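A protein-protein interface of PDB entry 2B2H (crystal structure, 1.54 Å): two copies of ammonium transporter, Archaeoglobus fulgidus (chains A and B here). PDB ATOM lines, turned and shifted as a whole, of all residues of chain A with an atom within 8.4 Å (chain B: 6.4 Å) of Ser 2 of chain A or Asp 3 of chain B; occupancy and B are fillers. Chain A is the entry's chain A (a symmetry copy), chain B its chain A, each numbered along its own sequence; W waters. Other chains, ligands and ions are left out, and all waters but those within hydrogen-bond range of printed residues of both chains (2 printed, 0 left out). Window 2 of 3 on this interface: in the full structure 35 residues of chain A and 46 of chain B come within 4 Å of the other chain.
Among the printed residues, merely in contact across the chains: Gly 4 of chain A with Asp 3 of chain B (3.6 Å), Gly 4 of chain A with Gly 4 of chain B (3.4 Å), Gly 4 of chain A with Ala 7 of chain B (3.4 Å), Trp 8 of chain A with Ala 7 of chain B (3.9 Å), Ala 212 of chain A with Asp 3 of chain B (3.4 Å), Ala 212 of chain A with Val 6 of chain B (3.5 Å) and Ala 212 of chain A with Ala 7 of chain B (3.7 Å).
Ser 2 of chain A touches Asp 3 of chain B, but with the chains exchanged Asp 3 of chain A does not touch Ser 2 of chain B (8.1 Å).
Gly 4 of chain A touches Asp 3 of chain B, but with the chains exchanged Asp 3 of chain A does not touch Gly 4 of chain B (5.4 Å).
Asn 5 of chain A touches Asp 3 of chain B, but with the chains exchanged Asp 3 of chain A does not touch Asn 5 of chain B (7.9 Å).
Trp 8 of chain A touches Ala 7 of chain B, but with the chains exchanged Ala 7 of chain A does not touch Trp 8 of chain B (6.3 Å).
8 positions are printed for both chains.
The side-chain carboxylate (OD2) of Asp 3 of chain B sits at hydrogen-bond distance from the side-chain hydroxyl (OG) of Ser 2 of chain A.
The side-chain carboxylate (OD2) of Asp 3 of chain B lies close to the side-chain amide oxygen (OD1) of Asn 5 of chain A (3.4 Å).
OD2 of Asp 214 of chain A sits close to SD of Met 1 of chain B (3.3 Å).
Of chain B, only Asp 3 (2.5 Å) comes within 4 Å of Ser 2 of chain A.
Printed residues of chain B within 4 Å of Gly 4 of chain A: Asp 3 (3.6 Å), Gly 4 (3.4 Å) and Ala 7 (3.4 Å).
Printed residues of chain B within 4 Å of Asn 5 of chain A: Asp 3.
Val 6 of chain A touches none of the printed residues of chain B.
Of the printed residues of chain B, Trp 8 of chain A touches Ala 7 (3.9 Å).
Ile 9 of chain A touches none of the printed residues of chain B.
Of the printed residues of chain B, Asp 214 of chain A touches Met 1.
Asp 3 of chain B touches four residues of chain A.
Gly 4 of chain B touches one residue of chain A.
Of the printed residues of chain A, Val 6 of chain B touches Ala 212.
Water W2 lies within hydrogen-bond range of the side-chain carboxylate of Asp 3 of chain B (2.5 Å) and the backbone carbonyl oxygen of Ala 212 of chain A (3.0 Å).
Water W1 bridges the side-chain amide oxygen (OD1) of Asn 5 of chain A (2.9 Å) and the side-chain carboxylate (OD1) of Asp 3 of chain B (2.9 Å).
Of the 16 printed residues of chain A, 6 touch a printed residue of chain B.
Hydrophobic or aromatic side chains of chain A within 4 Å of the printed part of chain B: Trp 8 and Ala 212.
Of the 8 printed residues of chain B, 5 touch a printed residue of chain A.
Hydrophobic or aromatic side chains of chain B within 4 Å of the printed part of chain A: Met 1, Val 6 and Ala 7.
Along chain B the printed residues that touch a printed residue of chain A span positions 1 to 7.
Among the printed residues, 10 pairs touch across the chains.
Among the printed residues, no Asp or Glu carboxylate lies within 4 Å of a Lys or Arg side-chain nitrogen of the other chain.
The side-chain hydroxyl (OG) of Ser 2 of chain A lies close to the backbone NH (N) of Asn 5 of chain A, at 3.4 Å.
N of Ala 212 of chain A sits at hydrogen-bond distance from OD1 of Asn 5 of chain A, 3.0 Å away.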
ATOM      1  N   MET A   1      -6.936  31.444  -2.713  1.00  0.00           N
ATOM      2  CA  MET A   1      -6.593  31.029  -1.310  1.00  0.00           C
ATOM      3  C   MET A   1      -6.864  29.544  -1.160  1.00  0.00           C
ATOM      4  O   MET A   1      -6.789  29.004  -0.060  1.00  0.00           O
ATOM      5  CB  MET A   1      -7.480  31.750  -0.289  1.00  0.00           C
ATOM      6  CG  MET A   1      -7.608  33.247  -0.415  1.00  0.00           C
ATOM      7  SD  MET A   1      -8.827  33.771   0.807  1.00  0.00           S
ATOM      8  CE  MET A   1     -10.363  33.325  -0.021  1.00  0.00           C
ATOM      9  N   SER A   2      -7.180  28.892  -2.272  1.00  0.00           N
ATOM     10  CA  SER A   2      -7.526  27.478  -2.259  1.00  0.00           C
ATOM     11  C   SER A   2      -8.961  27.466  -1.750  1.00  0.00           C
ATOM     12  O   SER A   2      -9.205  27.563  -0.543  1.00  0.00           O
ATOM     13  CB  SER A   2      -6.633  26.687  -1.302  1.00  0.00           C
ATOM     14  OG  SER A   2      -7.086  25.351  -1.207  1.00  0.00           O
ATOM     15  N   ASP A   3      -9.906  27.370  -2.681  1.00  0.00           N
ATOM     16  CA  ASP A   3     -11.319  27.365  -2.337  1.00  0.00           C
ATOM     17  C   ASP A   3     -11.631  26.211  -1.398  1.00  0.00           C
ATOM     18  O   ASP A   3     -12.463  26.340  -0.504  1.00  0.00           O
ATOM     19  CB  ASP A   3     -12.183  27.267  -3.598  1.00  0.00           C
ATOM     20  CG  ASP A   3     -11.860  28.358  -4.623  1.00  0.00           C
ATOM     21  OD1 ASP A   3     -11.404  29.457  -4.230  1.00  0.00           O
ATOM     22  OD2 ASP A   3     -12.078  28.115  -5.825  1.00  0.00           O
ATOM     23  N   GLY A   4     -10.946  25.089  -1.591  1.00  0.00           N
ATOM     24  CA  GLY A   4     -11.167  23.935  -0.739  1.00  0.00           C
ATOM     25  C   GLY A   4     -10.816  24.204   0.711  1.00  0.00           C
ATOM     26  O   GLY A   4     -11.560  23.806   1.609  1.00  0.00           O
ATOM     27  N   ASN A   5      -9.688  24.867   0.955  1.00  0.00           N
ATOM     28  CA  ASN A   5      -9.289  25.166   2.326  1.00  0.00           C
ATOM     29  C   ASN A   5     -10.252  26.148   2.979  1.00  0.00           C
ATOM     30  O   ASN A   5     -10.605  25.988   4.148  1.00  0.00           O
ATOM     31  CB  ASN A   5      -7.867  25.724   2.372  1.00  0.00           C
ATOM     32  CG  ASN A   5      -6.818  24.657   2.127  1.00  0.00           C
ATOM     33  OD1 ASN A   5      -7.133  23.464   2.056  1.00  0.00           O
ATOM     34  ND2 ASN A   5      -5.563  25.078   2.005  1.00  0.00           N
ATOM     35  N   VAL A   6     -10.675  27.167   2.235  1.00  0.00           N
ATOM     36  CA  VAL A   6     -11.628  28.128   2.781  1.00  0.00           C
ATOM     37  C   VAL A   6     -12.948  27.392   3.047  1.00  0.00           C
ATOM     38  O   VAL A   6     -13.609  27.635   4.052  1.00  0.00           O
ATOM     39  CB  VAL A   6     -11.882  29.310   1.801  1.00  0.00           C
ATOM     40  CG1 VAL A   6     -13.014  30.196   2.322  1.00  0.00           C
ATOM     41  CG2 VAL A   6     -10.612  30.127   1.645  1.00  0.00           C
ATOM     42  N   ALA A   7     -13.316  26.482   2.148  1.00  0.00           N
ATOM     43  CA  ALA A   7     -14.548  25.721   2.295  1.00  0.00           C
ATOM     44  C   ALA A   7     -14.552  24.933   3.596  1.00  0.00           C
ATOM     45  O   ALA A   7     -15.527  24.967   4.350  1.00  0.00           O
ATOM     46  CB  ALA A   7     -14.720  24.769   1.125  1.00  0.00           C
ATOM     47  N   TRP A   8     -13.458  24.227   3.861  1.00  0.00           N
ATOM     48  CA  TRP A   8     -13.372  23.431   5.069  1.00  0.00           C
ATOM     49  C   TRP A   8     -13.377  24.277   6.336  1.00  0.00           C
ATOM     50  O   TRP A   8     -13.999  23.901   7.325  1.00  0.00           O
ATOM     51  CB  TRP A   8     -12.125  22.549   5.041  1.00  0.00           C
ATOM     52  CG  TRP A   8     -11.969  21.730   6.277  1.00  0.00           C
ATOM     53  CD1 TRP A   8     -10.837  21.587   7.024  1.00  0.00           C
ATOM     54  CD2 TRP A   8     -12.984  20.955   6.936  1.00  0.00           C
ATOM     55  NE1 TRP A   8     -11.080  20.776   8.112  1.00  0.00           N
ATOM     56  CE2 TRP A   8     -12.390  20.376   8.083  1.00  0.00           C
ATOM     57  CE3 TRP A   8     -14.337  20.699   6.674  1.00  0.00           C
ATOM     58  CZ2 TRP A   8     -13.103  19.554   8.967  1.00  0.00           C
ATOM     59  CZ3 TRP A   8     -15.046  19.882   7.559  1.00  0.00           C
ATOM     60  CH2 TRP A   8     -14.426  19.323   8.689  1.00  0.00           C
ATOM     61  N   ILE A   9     -12.698  25.419   6.321  1.00  0.00           N
ATOM     62  CA  ILE A   9     -12.662  26.256   7.516  1.00  0.00           C
ATOM     63  C   ILE A   9     -13.951  27.038   7.728  1.00  0.00           C
ATOM     64  O   ILE A   9     -14.305  27.350   8.869  1.00  0.00           O
ATOM     65  CB  ILE A   9     -11.457  27.215   7.501  1.00  0.00           C
ATOM     66  CG1 ILE A   9     -10.167  26.392   7.422  1.00  0.00           C
ATOM     67  CG2 ILE A   9     -11.438  28.062   8.764  1.00  0.00           C
ATOM     68  CD1 ILE A   9     -10.084  25.263   8.462  1.00  0.00           C
ATOM     69  N   GLU A  85      -8.010  36.049   4.462  1.00  0.00           N
ATOM     70  CA  GLU A  85      -7.978  34.846   5.287  1.00  0.00           C
ATOM     71  C   GLU A  85      -7.862  35.143   6.773  1.00  0.00           C
ATOM     72  O   GLU A  85      -8.243  34.316   7.597  1.00  0.00           O
ATOM     73  CB  GLU A  85      -6.828  33.924   4.868  1.00  0.00           C
ATOM     74  CG  GLU A  85      -6.917  33.428   3.429  1.00  0.00           C
ATOM     75  CD  GLU A  85      -6.007  32.235   3.149  1.00  0.00           C
ATOM     76  OE1 GLU A  85      -4.858  32.224   3.650  1.00  0.00           O
ATOM     77  OE2 GLU A  85      -6.439  31.315   2.416  1.00  0.00           O
ATOM     78  N   LEU A  88     -11.146  34.996   8.254  1.00  0.00           N
ATOM     79  CA  LEU A  88     -11.669  33.654   8.471  1.00  0.00           C
ATOM     80  C   LEU A  88     -11.039  33.063   9.723  1.00  0.00           C
ATOM     81  O   LEU A  88     -11.710  32.371  10.488  1.00  0.00           O
ATOM     82  CB  LEU A  88     -11.404  32.750   7.260  1.00  0.00           C
ATOM     83  CG  LEU A  88     -11.989  31.334   7.378  1.00  0.00           C
ATOM     84  CD1 LEU A  88     -13.411  31.391   7.901  1.00  0.00           C
ATOM     85  CD2 LEU A  88     -11.954  30.658   6.028  1.00  0.00           C
ATOM     86  N   LEU A 210      -6.217  24.221   9.661  1.00  0.00           N
ATOM     87  CA  LEU A 210      -6.470  25.401   8.844  1.00  0.00           C
ATOM     88  C   LEU A 210      -6.401  25.113   7.350  1.00  0.00           C
ATOM     89  O   LEU A 210      -6.087  25.991   6.545  1.00  0.00           O
ATOM     90  CB  LEU A 210      -5.501  26.517   9.228  1.00  0.00           C
ATOM     91  CG  LEU A 210      -5.613  26.940  10.698  1.00  0.00           C
ATOM     92  CD1 LEU A 210      -4.676  28.101  10.952  1.00  0.00           C
ATOM     93  CD2 LEU A 210      -7.038  27.349  11.026  1.00  0.00           C
ATOM     94  N   ALA A 211      -6.717  23.875   6.990  1.00  0.00           N
ATOM     95  CA  ALA A 211      -6.704  23.438   5.601  1.00  0.00           C
ATOM     96  C   ALA A 211      -7.292  22.040   5.517  1.00  0.00           C
ATOM     97  O   ALA A 211      -7.286  21.297   6.502  1.00  0.00           O
ATOM     98  CB  ALA A 211      -5.281  23.429   5.062  1.00  0.00           C
ATOM     99  N   ALA A 212      -7.804  21.689   4.339  1.00  0.00           N
ATOM    100  CA  ALA A 212      -8.392  20.372   4.120  1.00  0.00           C
ATOM    101  C   ALA A 212      -7.259  19.504   3.609  1.00  0.00           C
ATOM    102  O   ALA A 212      -7.190  19.200   2.426  1.00  0.00           O
ATOM    103  CB  ALA A 212      -9.510  20.462   3.085  1.00  0.00           C
ATOM    104  N   ASN A 213      -6.369  19.114   4.515  1.00  0.00           N
ATOM    105  CA  ASN A 213      -5.205  18.314   4.153  1.00  0.00           C
ATOM    106  C   ASN A 213      -5.055  17.038   4.975  1.00  0.00           C
ATOM    107  O   ASN A 213      -5.969  16.634   5.701  1.00  0.00           O
ATOM    108  CB  ASN A 213      -3.939  19.173   4.298  1.00  0.00           C
ATOM    109  CG  ASN A 213      -3.708  19.655   5.732  1.00  0.00           C
ATOM    110  OD1 ASN A 213      -2.821  20.473   5.993  1.00  0.00           O
ATOM    111  ND2 ASN A 213      -4.502  19.147   6.666  1.00  0.00           N
ATOM    112  N   ASP A 214      -3.885  16.408   4.863  1.00  0.00           N
ATOM    113  CA  ASP A 214      -3.601  15.174   5.596  1.00  0.00           C
ATOM    114  C   ASP A 214      -3.587  15.365   7.122  1.00  0.00           C
ATOM    115  O   ASP A 214      -3.874  14.422   7.864  1.00  0.00           O
ATOM    116  CB  ASP A 214      -2.268  14.563   5.122  1.00  0.00           C
ATOM    117  CG  ASP A 214      -2.403  13.795   3.799  1.00  0.00           C
ATOM    118  OD1 ASP A 214      -1.368  13.337   3.260  1.00  0.00           O
ATOM    119  OD2 ASP A 214      -3.540  13.639   3.302  1.00  0.00           O
ATOM    120  N   MET B   1      -4.376  16.790  -3.270  1.00  0.00           N
ATOM    121  CA  MET B   1      -5.487  15.779  -3.337  1.00  0.00           C
ATOM    122  C   MET B   1      -6.777  16.494  -3.692  1.00  0.00           C
ATOM    123  O   MET B   1      -7.849  15.896  -3.670  1.00  0.00           O
ATOM    124  CB  MET B   1      -5.708  15.111  -1.974  1.00  0.00           C
ATOM    125  CG  MET B   1      -4.495  14.566  -1.264  1.00  0.00           C
ATOM    126  SD  MET B   1      -5.050  14.000   0.356  1.00  0.00           S
ATOM    127  CE  MET B   1      -5.170  15.563   1.246  1.00  0.00           C
ATOM    128  N   SER B   2      -6.664  17.776  -4.019  1.00  0.00           N
ATOM    129  CA  SER B   2      -7.830  18.594  -4.320  1.00  0.00           C
ATOM    130  C   SER B   2      -8.406  18.914  -2.947  1.00  0.00           C
ATOM    131  O   SER B   2      -9.106  18.091  -2.348  1.00  0.00           O
ATOM    132  CB  SER B   2      -8.861  17.826  -5.147  1.00  0.00           C
ATOM    133  OG  SER B   2     -10.035  18.599  -5.299  1.00  0.00           O
ATOM    134  N   ASP B   3      -8.085  20.102  -2.444  1.00  0.00           N
ATOM    135  CA  ASP B   3      -8.552  20.530  -1.136  1.00  0.00           C
ATOM    136  C   ASP B   3     -10.072  20.525  -1.089  1.00  0.00           C
ATOM    137  O   ASP B   3     -10.664  20.202  -0.062  1.00  0.00           O
ATOM    138  CB  ASP B   3      -8.019  21.926  -0.800  1.00  0.00           C
ATOM    139  CG  ASP B   3      -6.495  22.020  -0.908  1.00  0.00           C
ATOM    140  OD1 ASP B   3      -5.800  20.994  -0.720  1.00  0.00           O
ATOM    141  OD2 ASP B   3      -5.993  23.128  -1.171  1.00  0.00           O
ATOM    142  N   GLY B   4     -10.701  20.864  -2.209  1.00  0.00           N
ATOM    143  CA  GLY B   4     -12.151  20.880  -2.264  1.00  0.00           C
ATOM    144  C   GLY B   4     -12.759  19.510  -2.033  1.00  0.00           C
ATOM    145  O   GLY B   4     -13.745  19.388  -1.305  1.00  0.00           O
ATOM    146  N   ASN B   5     -12.190  18.476  -2.649  1.00  0.00           N
ATOM    147  CA  ASN B   5     -12.718  17.128  -2.470  1.00  0.00           C
ATOM    148  C   ASN B   5     -12.528  16.647  -1.037  1.00  0.00           C
ATOM    149  O   ASN B   5     -13.423  16.026  -0.465  1.00  0.00           O
ATOM    150  CB  ASN B   5     -12.057  16.148  -3.438  1.00  0.00           C
ATOM    151  CG  ASN B   5     -12.546  16.325  -4.863  1.00  0.00           C
ATOM    152  OD1 ASN B   5     -13.484  17.087  -5.121  1.00  0.00           O
ATOM    153  ND2 ASN B   5     -11.921  15.614  -5.795  1.00  0.00           N
ATOM    154  N   VAL B   6     -11.363  16.925  -0.454  1.00  0.00           N
ATOM    155  CA  VAL B   6     -11.122  16.529   0.929  1.00  0.00           C
ATOM    156  C   VAL B   6     -12.091  17.312   1.825  1.00  0.00           C
ATOM    157  O   VAL B   6     -12.631  16.772   2.784  1.00  0.00           O
ATOM    158  CB  VAL B   6      -9.658  16.823   1.367  1.00  0.00           C
ATOM    159  CG1 VAL B   6      -9.491  16.567   2.865  1.00  0.00           C
ATOM    160  CG2 VAL B   6      -8.702  15.945   0.580  1.00  0.00           C
ATOM    161  N   ALA B   7     -12.316  18.580   1.494  1.00  0.00           N
ATOM    162  CA  ALA B   7     -13.217  19.422   2.270  1.00  0.00           C
ATOM    163  C   ALA B   7     -14.617  18.828   2.313  1.00  0.00           C
ATOM    164  O   ALA B   7     -15.223  18.723   3.382  1.00  0.00           O
ATOM    165  CB  ALA B   7     -13.276  20.817   1.676  1.00  0.00           C
ATOM    166  N   TRP B   8     -15.127  18.437   1.151  1.00  0.00           N
ATOM    167  CA  TRP B   8     -16.461  17.873   1.086  1.00  0.00           C
ATOM    168  C   TRP B   8     -16.575  16.540   1.816  1.00  0.00           C
ATOM    169  O   TRP B   8     -17.578  16.283   2.475  1.00  0.00           O
ATOM    170  CB  TRP B   8     -16.902  17.706  -0.367  1.00  0.00           C
ATOM    171  CG  TRP B   8     -18.258  17.099  -0.493  1.00  0.00           C
ATOM    172  CD1 TRP B   8     -18.617  16.067  -1.309  1.00  0.00           C
ATOM    173  CD2 TRP B   8     -19.440  17.462   0.239  1.00  0.00           C
ATOM    174  NE1 TRP B   8     -19.949  15.759  -1.132  1.00  0.00           N
ATOM    175  CE2 TRP B   8     -20.478  16.598  -0.187  1.00  0.00           C
ATOM    176  CE3 TRP B   8     -19.724  18.427   1.215  1.00  0.00           C
ATOM    177  CZ2 TRP B   8     -21.779  16.670   0.331  1.00  0.00           C
ATOM    178  CZ3 TRP B   8     -21.021  18.496   1.731  1.00  0.00           C
ATOM    179  CH2 TRP B   8     -22.028  17.621   1.286  1.00  0.00           C
HETATM  180  O   HOH W   1      -4.793  21.721   1.927  1.00  0.00           O
HETATM  181  O   HOH W   2      -5.614  18.590  -0.021  1.00  0.00           O
